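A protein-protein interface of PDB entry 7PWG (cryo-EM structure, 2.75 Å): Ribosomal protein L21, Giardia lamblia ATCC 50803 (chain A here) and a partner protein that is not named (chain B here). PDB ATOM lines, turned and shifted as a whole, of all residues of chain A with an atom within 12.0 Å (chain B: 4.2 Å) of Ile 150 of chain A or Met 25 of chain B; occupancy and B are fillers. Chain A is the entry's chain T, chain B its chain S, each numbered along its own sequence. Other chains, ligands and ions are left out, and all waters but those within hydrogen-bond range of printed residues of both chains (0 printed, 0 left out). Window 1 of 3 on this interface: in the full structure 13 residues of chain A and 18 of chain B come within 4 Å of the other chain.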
ATOM      1  N   ILE A 144     -26.577   4.678  -3.718  1.00  0.00           N
ATOM      2  CA  ILE A 144     -25.608   5.072  -4.735  1.00  0.00           C
ATOM      3  C   ILE A 144     -25.310   6.562  -4.637  1.00  0.00           C
ATOM      4  O   ILE A 144     -25.017   7.212  -5.644  1.00  0.00           O
ATOM      5  CB  ILE A 144     -26.087   4.720  -6.152  1.00  0.00           C
ATOM      6  CG1 ILE A 144     -27.382   5.475  -6.472  1.00  0.00           C
ATOM      7  CG2 ILE A 144     -26.220   3.218  -6.310  1.00  0.00           C
ATOM      8  CD1 ILE A 144     -28.082   4.982  -7.693  1.00  0.00           C
ATOM      9  N   SER A 146     -22.645   7.876  -3.179  1.00  0.00           N
ATOM     10  CA  SER A 146     -21.220   7.947  -3.488  1.00  0.00           C
ATOM     11  C   SER A 146     -20.863   6.753  -4.367  1.00  0.00           C
ATOM     12  O   SER A 146     -20.689   5.641  -3.871  1.00  0.00           O
ATOM     13  CB  SER A 146     -20.401   7.960  -2.202  1.00  0.00           C
ATOM     14  OG  SER A 146     -19.020   7.884  -2.480  1.00  0.00           O
ATOM     15  N   ALA A 147     -20.743   6.989  -5.667  1.00  0.00           N
ATOM     16  CA  ALA A 147     -20.442   5.950  -6.638  1.00  0.00           C
ATOM     17  C   ALA A 147     -19.168   6.303  -7.391  1.00  0.00           C
ATOM     18  O   ALA A 147     -18.968   7.459  -7.774  1.00  0.00           O
ATOM     19  CB  ALA A 147     -21.595   5.771  -7.616  1.00  0.00           C
ATOM     20  N   ILE A 148     -18.303   5.305  -7.588  1.00  0.00           N
ATOM     21  CA  ILE A 148     -17.021   5.478  -8.264  1.00  0.00           C
ATOM     22  C   ILE A 148     -17.183   5.102  -9.728  1.00  0.00           C
ATOM     23  O   ILE A 148     -17.938   4.189 -10.079  1.00  0.00           O
ATOM     24  CB  ILE A 148     -15.906   4.639  -7.602  1.00  0.00           C
ATOM     25  CG1 ILE A 148     -16.066   4.637  -6.086  1.00  0.00           C
ATOM     26  CG2 ILE A 148     -14.549   5.200  -7.941  1.00  0.00           C
ATOM     27  CD1 ILE A 148     -15.975   6.010  -5.469  1.00  0.00           C
ATOM     28  N   ASP A 149     -16.464   5.808 -10.596  1.00  0.00           N
ATOM     29  CA  ASP A 149     -16.600   5.662 -12.044  1.00  0.00           C
ATOM     30  C   ASP A 149     -15.279   5.183 -12.609  1.00  0.00           C
ATOM     31  O   ASP A 149     -14.336   5.967 -12.736  1.00  0.00           O
ATOM     32  CB  ASP A 149     -17.024   6.976 -12.689  1.00  0.00           C
ATOM     33  CG  ASP A 149     -18.094   7.685 -11.893  1.00  0.00           C
ATOM     34  OD1 ASP A 149     -18.983   6.989 -11.372  1.00  0.00           O
ATOM     35  OD2 ASP A 149     -18.028   8.925 -11.765  1.00  0.00           O
ATOM     36  N   ILE A 150     -15.210   3.906 -12.969  1.00  0.00           N
ATOM     37  CA  ILE A 150     -14.008   3.334 -13.536  1.00  0.00           C
ATOM     38  C   ILE A 150     -14.219   3.057 -15.018  1.00  0.00           C
ATOM     39  O   ILE A 150     -15.323   3.148 -15.544  1.00  0.00           O
ATOM     40  CB  ILE A 150     -13.551   2.069 -12.789  1.00  0.00           C
ATOM     41  CG1 ILE A 150     -14.656   1.032 -12.689  1.00  0.00           C
ATOM     42  CG2 ILE A 150     -13.053   2.426 -11.412  1.00  0.00           C
ATOM     43  CD1 ILE A 150     -14.200  -0.192 -11.936  1.00  0.00           C
ATOM     44  N   THR A 151     -13.122   2.738 -15.689  1.00  0.00           N
ATOM     45  CA  THR A 151     -13.057   2.546 -17.129  1.00  0.00           C
ATOM     46  C   THR A 151     -11.787   1.767 -17.437  1.00  0.00           C
ATOM     47  O   THR A 151     -10.860   1.749 -16.622  1.00  0.00           O
ATOM     48  CB  THR A 151     -13.045   3.893 -17.870  1.00  0.00           C
ATOM     49  OG1 THR A 151     -12.466   4.901 -17.032  1.00  0.00           O
ATOM     50  CG2 THR A 151     -14.451   4.306 -18.309  1.00  0.00           C
ATOM     51  N   PRO A 152     -11.702   1.136 -18.605  1.00  0.00           N
ATOM     52  CA  PRO A 152     -10.453   0.472 -18.993  1.00  0.00           C
ATOM     53  C   PRO A 152      -9.300   1.457 -19.129  1.00  0.00           C
ATOM     54  O   PRO A 152      -9.492   2.643 -19.392  1.00  0.00           O
ATOM     55  CB  PRO A 152     -10.798  -0.160 -20.342  1.00  0.00           C
ATOM     56  CG  PRO A 152     -12.253  -0.298 -20.321  1.00  0.00           C
ATOM     57  CD  PRO A 152     -12.787   0.832 -19.541  1.00  0.00           C
ATOM     58  N   LEU A 153      -8.088   0.951 -18.944  1.00  0.00           N
ATOM     59  CA  LEU A 153      -6.876   1.752 -18.991  1.00  0.00           C
ATOM     60  C   LEU A 153      -6.096   1.488 -20.274  1.00  0.00           C
ATOM     61  O   LEU A 153      -6.322   0.505 -20.977  1.00  0.00           O
ATOM     62  CB  LEU A 153      -6.003   1.460 -17.772  1.00  0.00           C
ATOM     63  CG  LEU A 153      -6.461   2.027 -16.434  1.00  0.00           C
ATOM     64  CD1 LEU A 153      -5.760   1.306 -15.318  1.00  0.00           C
ATOM     65  CD2 LEU A 153      -6.163   3.497 -16.378  1.00  0.00           C
ATOM     66  N   LYS A 154      -5.153   2.376 -20.567  1.00  0.00           N
ATOM     67  CA  LYS A 154      -4.356   2.257 -21.778  1.00  0.00           C
ATOM     68  C   LYS A 154      -3.181   1.308 -21.582  1.00  0.00           C
ATOM     69  O   LYS A 154      -2.639   1.170 -20.484  1.00  0.00           O
ATOM     70  CB  LYS A 154      -3.834   3.618 -22.219  1.00  0.00           C
ATOM     71  CG  LYS A 154      -2.873   4.230 -21.249  1.00  0.00           C
ATOM     72  CD  LYS A 154      -2.424   5.593 -21.694  1.00  0.00           C
ATOM     73  CE  LYS A 154      -1.532   5.516 -22.917  1.00  0.00           C
ATOM     74  NZ  LYS A 154      -0.954   6.855 -23.224  1.00  0.00           N
ATOM     75  N   TYR B   5     -25.514   0.717 -22.302  1.00  0.00           N
ATOM     76  CA  TYR B   5     -25.935   0.221 -20.999  1.00  0.00           C
ATOM     77  C   TYR B   5     -25.091   0.852 -19.898  1.00  0.00           C
ATOM     78  O   TYR B   5     -23.902   1.099 -20.079  1.00  0.00           O
ATOM     79  CB  TYR B   5     -25.811  -1.304 -20.881  1.00  0.00           C
ATOM     80  CG  TYR B   5     -26.712  -2.119 -21.768  1.00  0.00           C
ATOM     81  CD1 TYR B   5     -28.025  -2.357 -21.419  1.00  0.00           C
ATOM     82  CD2 TYR B   5     -26.238  -2.673 -22.944  1.00  0.00           C
ATOM     83  CE1 TYR B   5     -28.832  -3.104 -22.216  1.00  0.00           C
ATOM     84  CE2 TYR B   5     -27.044  -3.415 -23.744  1.00  0.00           C
ATOM     85  CZ  TYR B   5     -28.340  -3.638 -23.375  1.00  0.00           C
ATOM     86  OH  TYR B   5     -29.166  -4.385 -24.180  1.00  0.00           O
ATOM     87  N   ILE B   6     -25.715   1.094 -18.749  1.00  0.00           N
ATOM     88  CA  ILE B   6     -25.034   1.562 -17.546  1.00  0.00           C
ATOM     89  C   ILE B   6     -25.168   0.490 -16.477  1.00  0.00           C
ATOM     90  O   ILE B   6     -26.286   0.126 -16.103  1.00  0.00           O
ATOM     91  CB  ILE B   6     -25.600   2.894 -17.034  1.00  0.00           C
ATOM     92  CG1 ILE B   6     -25.305   4.025 -18.008  1.00  0.00           C
ATOM     93  CG2 ILE B   6     -25.005   3.238 -15.688  1.00  0.00           C
ATOM     94  CD1 ILE B   6     -25.749   5.373 -17.488  1.00  0.00           C
ATOM     95  N   VAL B   7     -24.037   0.017 -15.950  1.00  0.00           N
ATOM     96  CA  VAL B   7     -24.026  -1.086 -14.997  1.00  0.00           C
ATOM     97  C   VAL B   7     -23.440  -0.630 -13.668  1.00  0.00           C
ATOM     98  O   VAL B   7     -22.432   0.077 -13.634  1.00  0.00           O
ATOM     99  CB  VAL B   7     -23.252  -2.301 -15.540  1.00  0.00           C
ATOM    100  CG1 VAL B   7     -23.525  -3.491 -14.702  1.00  0.00           C
ATOM    101  CG2 VAL B   7     -23.632  -2.584 -16.955  1.00  0.00           C
ATOM    102  N   ARG B  24     -19.665   2.064 -11.173  1.00  0.00           N
ATOM    103  CA  ARG B  24     -20.549   2.146 -12.326  1.00  0.00           C
ATOM    104  C   ARG B  24     -19.738   2.279 -13.610  1.00  0.00           C
ATOM    105  O   ARG B  24     -18.626   2.809 -13.606  1.00  0.00           O
ATOM    106  CB  ARG B  24     -21.552   3.306 -12.195  1.00  0.00           C
ATOM    107  CG  ARG B  24     -21.068   4.653 -12.658  1.00  0.00           C
ATOM    108  CD  ARG B  24     -22.212   5.575 -13.038  1.00  0.00           C
ATOM    109  NE  ARG B  24     -22.971   6.054 -11.881  1.00  0.00           N
ATOM    110  CZ  ARG B  24     -22.665   7.140 -11.176  1.00  0.00           C
ATOM    111  NH1 ARG B  24     -21.606   7.874 -11.491  1.00  0.00           N
ATOM    112  NH2 ARG B  24     -23.410   7.487 -10.139  1.00  0.00           N
ATOM    113  N   MET B  25     -20.297   1.762 -14.706  1.00  0.00           N
ATOM    114  CA  MET B  25     -19.653   1.796 -16.012  1.00  0.00           C
ATOM    115  C   MET B  25     -20.682   2.025 -17.106  1.00  0.00           C
ATOM    116  O   MET B  25     -21.862   1.708 -16.965  1.00  0.00           O
ATOM    117  CB  MET B  25     -18.894   0.500 -16.332  1.00  0.00           C
ATOM    118  CG  MET B  25     -17.613   0.261 -15.546  1.00  0.00           C
ATOM    119  SD  MET B  25     -16.789  -1.274 -15.991  1.00  0.00           S
ATOM    120  CE  MET B  25     -15.263  -0.666 -16.714  1.00  0.00           C
ATOM    121  N   THR B  26     -20.207   2.556 -18.221  1.00  0.00           N
ATOM    122  CA  THR B  26     -20.966   2.621 -19.455  1.00  0.00           C
ATOM    123  C   THR B  26     -20.435   1.555 -20.404  1.00  0.00           C
ATOM    124  O   THR B  26     -19.230   1.484 -20.636  1.00  0.00           O
ATOM    125  CB  THR B  26     -20.872   4.015 -20.073  1.00  0.00           C
ATOM    126  OG1 THR B  26     -21.513   4.950 -19.204  1.00  0.00           O
ATOM    127  CG2 THR B  26     -21.567   4.068 -21.420  1.00  0.00           C
ATOM    128  N   ILE B  27     -21.332   0.713 -20.920  1.00  0.00           N
ATOM    129  CA  ILE B  27     -20.984  -0.443 -21.742  1.00  0.00           C
ATOM    130  C   ILE B  27     -21.779  -0.394 -23.041  1.00  0.00           C
ATOM    131  O   ILE B  27     -22.929   0.046 -23.052  1.00  0.00           O
ATOM    132  CB  ILE B  27     -21.262  -1.773 -21.012  1.00  0.00           C
ATOM    133  CG1 ILE B  27     -20.846  -1.708 -19.546  1.00  0.00           C
ATOM    134  CG2 ILE B  27     -20.577  -2.926 -21.711  1.00  0.00           C
ATOM    135  CD1 ILE B  27     -19.445  -2.085 -19.282  1.00  0.00           C
ATOM    136  N   PHE B  39     -18.971  -6.248 -17.931  1.00  0.00           N
ATOM    137  CA  PHE B  39     -18.762  -5.524 -16.682  1.00  0.00           C
ATOM    138  C   PHE B  39     -17.914  -6.326 -15.707  1.00  0.00           C
ATOM    139  O   PHE B  39     -17.108  -5.754 -14.968  1.00  0.00           O
ATOM    140  CB  PHE B  39     -20.107  -5.163 -16.046  1.00  0.00           C
ATOM    141  CG  PHE B  39     -19.983  -4.473 -14.717  1.00  0.00           C
ATOM    142  CD1 PHE B  39     -19.836  -3.096 -14.643  1.00  0.00           C
ATOM    143  CD2 PHE B  39     -19.983  -5.199 -13.540  1.00  0.00           C
ATOM    144  CE1 PHE B  39     -19.704  -2.469 -13.424  1.00  0.00           C
ATOM    145  CE2 PHE B  39     -19.862  -4.572 -12.327  1.00  0.00           C
ATOM    146  CZ  PHE B  39     -19.722  -3.207 -12.269  1.00  0.00           C
ATOM    147  N   HIS B  42     -13.999  -6.313 -16.539  1.00  0.00           N
ATOM    148  CA  HIS B  42     -13.213  -5.164 -16.102  1.00  0.00           C
ATOM    149  C   HIS B  42     -13.111  -5.071 -14.590  1.00  0.00           C
ATOM    150  O   HIS B  42     -12.033  -4.809 -14.065  1.00  0.00           O
ATOM    151  CB  HIS B  42     -13.811  -3.865 -16.646  1.00  0.00           C
ATOM    152  CG  HIS B  42     -13.755  -3.747 -18.134  1.00  0.00           C
ATOM    153  ND1 HIS B  42     -12.572  -3.736 -18.836  1.00  0.00           N
ATOM    154  CD2 HIS B  42     -14.739  -3.638 -19.056  1.00  0.00           C
ATOM    155  CE1 HIS B  42     -12.829  -3.633 -20.126  1.00  0.00           C
ATOM    156  NE2 HIS B  42     -14.135  -3.569 -20.286  1.00  0.00           N
ATOM    157  N   LEU B  43     -14.211  -5.289 -13.872  1.00  0.00           N
ATOM    158  CA  LEU B  43     -14.184  -5.217 -12.418  1.00  0.00           C
ATOM    159  C   LEU B  43     -13.276  -6.273 -11.800  1.00  0.00           C
ATOM    160  O   LEU B  43     -12.875  -6.126 -10.647  1.00  0.00           O
ATOM    161  CB  LEU B  43     -15.603  -5.350 -11.861  1.00  0.00           C
ATOM    162  CG  LEU B  43     -15.735  -4.793 -10.447  1.00  0.00           C
ATOM    163  CD1 LEU B  43     -15.101  -3.433 -10.432  1.00  0.00           C
ATOM    164  CD2 LEU B  43     -17.161  -4.687  -9.996  1.00  0.00           C
ATOM    165  N   LYS B  47     -10.395  -3.915 -10.258  1.00  0.00           N
ATOM    166  CA  LYS B  47     -10.677  -3.898  -8.836  1.00  0.00           C
ATOM    167  C   LYS B  47     -10.593  -5.263  -8.176  1.00  0.00           C
ATOM    168  O   LYS B  47     -10.835  -5.357  -6.974  1.00  0.00           O
ATOM    169  CB  LYS B  47     -12.053  -3.289  -8.573  1.00  0.00           C
ATOM    170  CG  LYS B  47     -12.156  -1.806  -8.919  1.00  0.00           C
ATOM    171  CD  LYS B  47     -11.460  -0.942  -7.878  1.00  0.00           C
ATOM    172  CE  LYS B  47     -10.975   0.355  -8.479  1.00  0.00           C
ATOM    173  NZ  LYS B  47     -10.363   1.238  -7.477  1.00  0.00           N
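The backbone NH of Arg 24 of chain B lies within hydrogen-bond range of the backbone carbonyl oxygen of Ile 148 of chain A, 2.9 Å away. OD1 of Asp 149 of chain A is in salt-bridge range of NH1 of Arg 24 of chain B, 2.8 Å away.
The backbone carbonyl oxygen (O) of Val 7 of chain B lies within hydrogen-bond range of the backbone NH (N) of Met 25 of chain B (2.9 Å).
Among the printed residues, merely in contact across the chains: Ala 147 of chain A with Arg 24 of chain B (3.6 Å), Ile 150 of chain A with Arg 24 of chain B (3.6 Å), Ile 150 of chain A with Met 25 of chain B (3.7 Å), Ile 150 of chain A with Leu 43 of chain B (3.7 Å), Ile 150 of chain A with Lys 47 of chain B (3.99 Å), Thr 151 of chain A with Met 25 of chain B (3.9 Å) and Pro 152 of chain A with His 42 of chain B (3.4 Å).
Printed residues of chain B within 4 Å of Ala 147 of chain A: Arg 24. Printed residues of chain B within 4 Å of Ile 150 of chain A: Arg 24, Met 25, Leu 43 and Lys 47. Printed residues of chain B within 4 Å of Thr 151 of chain A: Met 25. Leu 153 of chain A touches none of the printed residues of chain B. No residue of chain A comes within 4 Å of Ile 6 of chain B. No residue of chain A comes within 4 Å of Val 7 of chain B. Printed residues of chain A within 4 Å of Arg 24 of chain B: Ala 147 (3.6 Å), Ile 148 (2.9 Å), Asp 149 (2.8 Å) and Ile 150 (3.6 Å). Of chain A, only Ile 150 and Thr 151 come within 4 Å of Met 25 of chain B. Thr 26 of chain B touches none of the printed residues of chain A. No residue of chain A comes within 4 Å of Ile 27 of chain B. The nearest printed residue of chain B that does not touch Thr 151 of chain A is His 42 of chain B (5.7 Å).
Of the 10 printed residues of chain A, 6 touch a printed residue of chain B. Among the printed residues, Asp or Glu carboxylates within 4 Å of a Lys or Arg side-chain nitrogen of the other chain: Asp 149 of chain A with Arg 24 of chain B.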
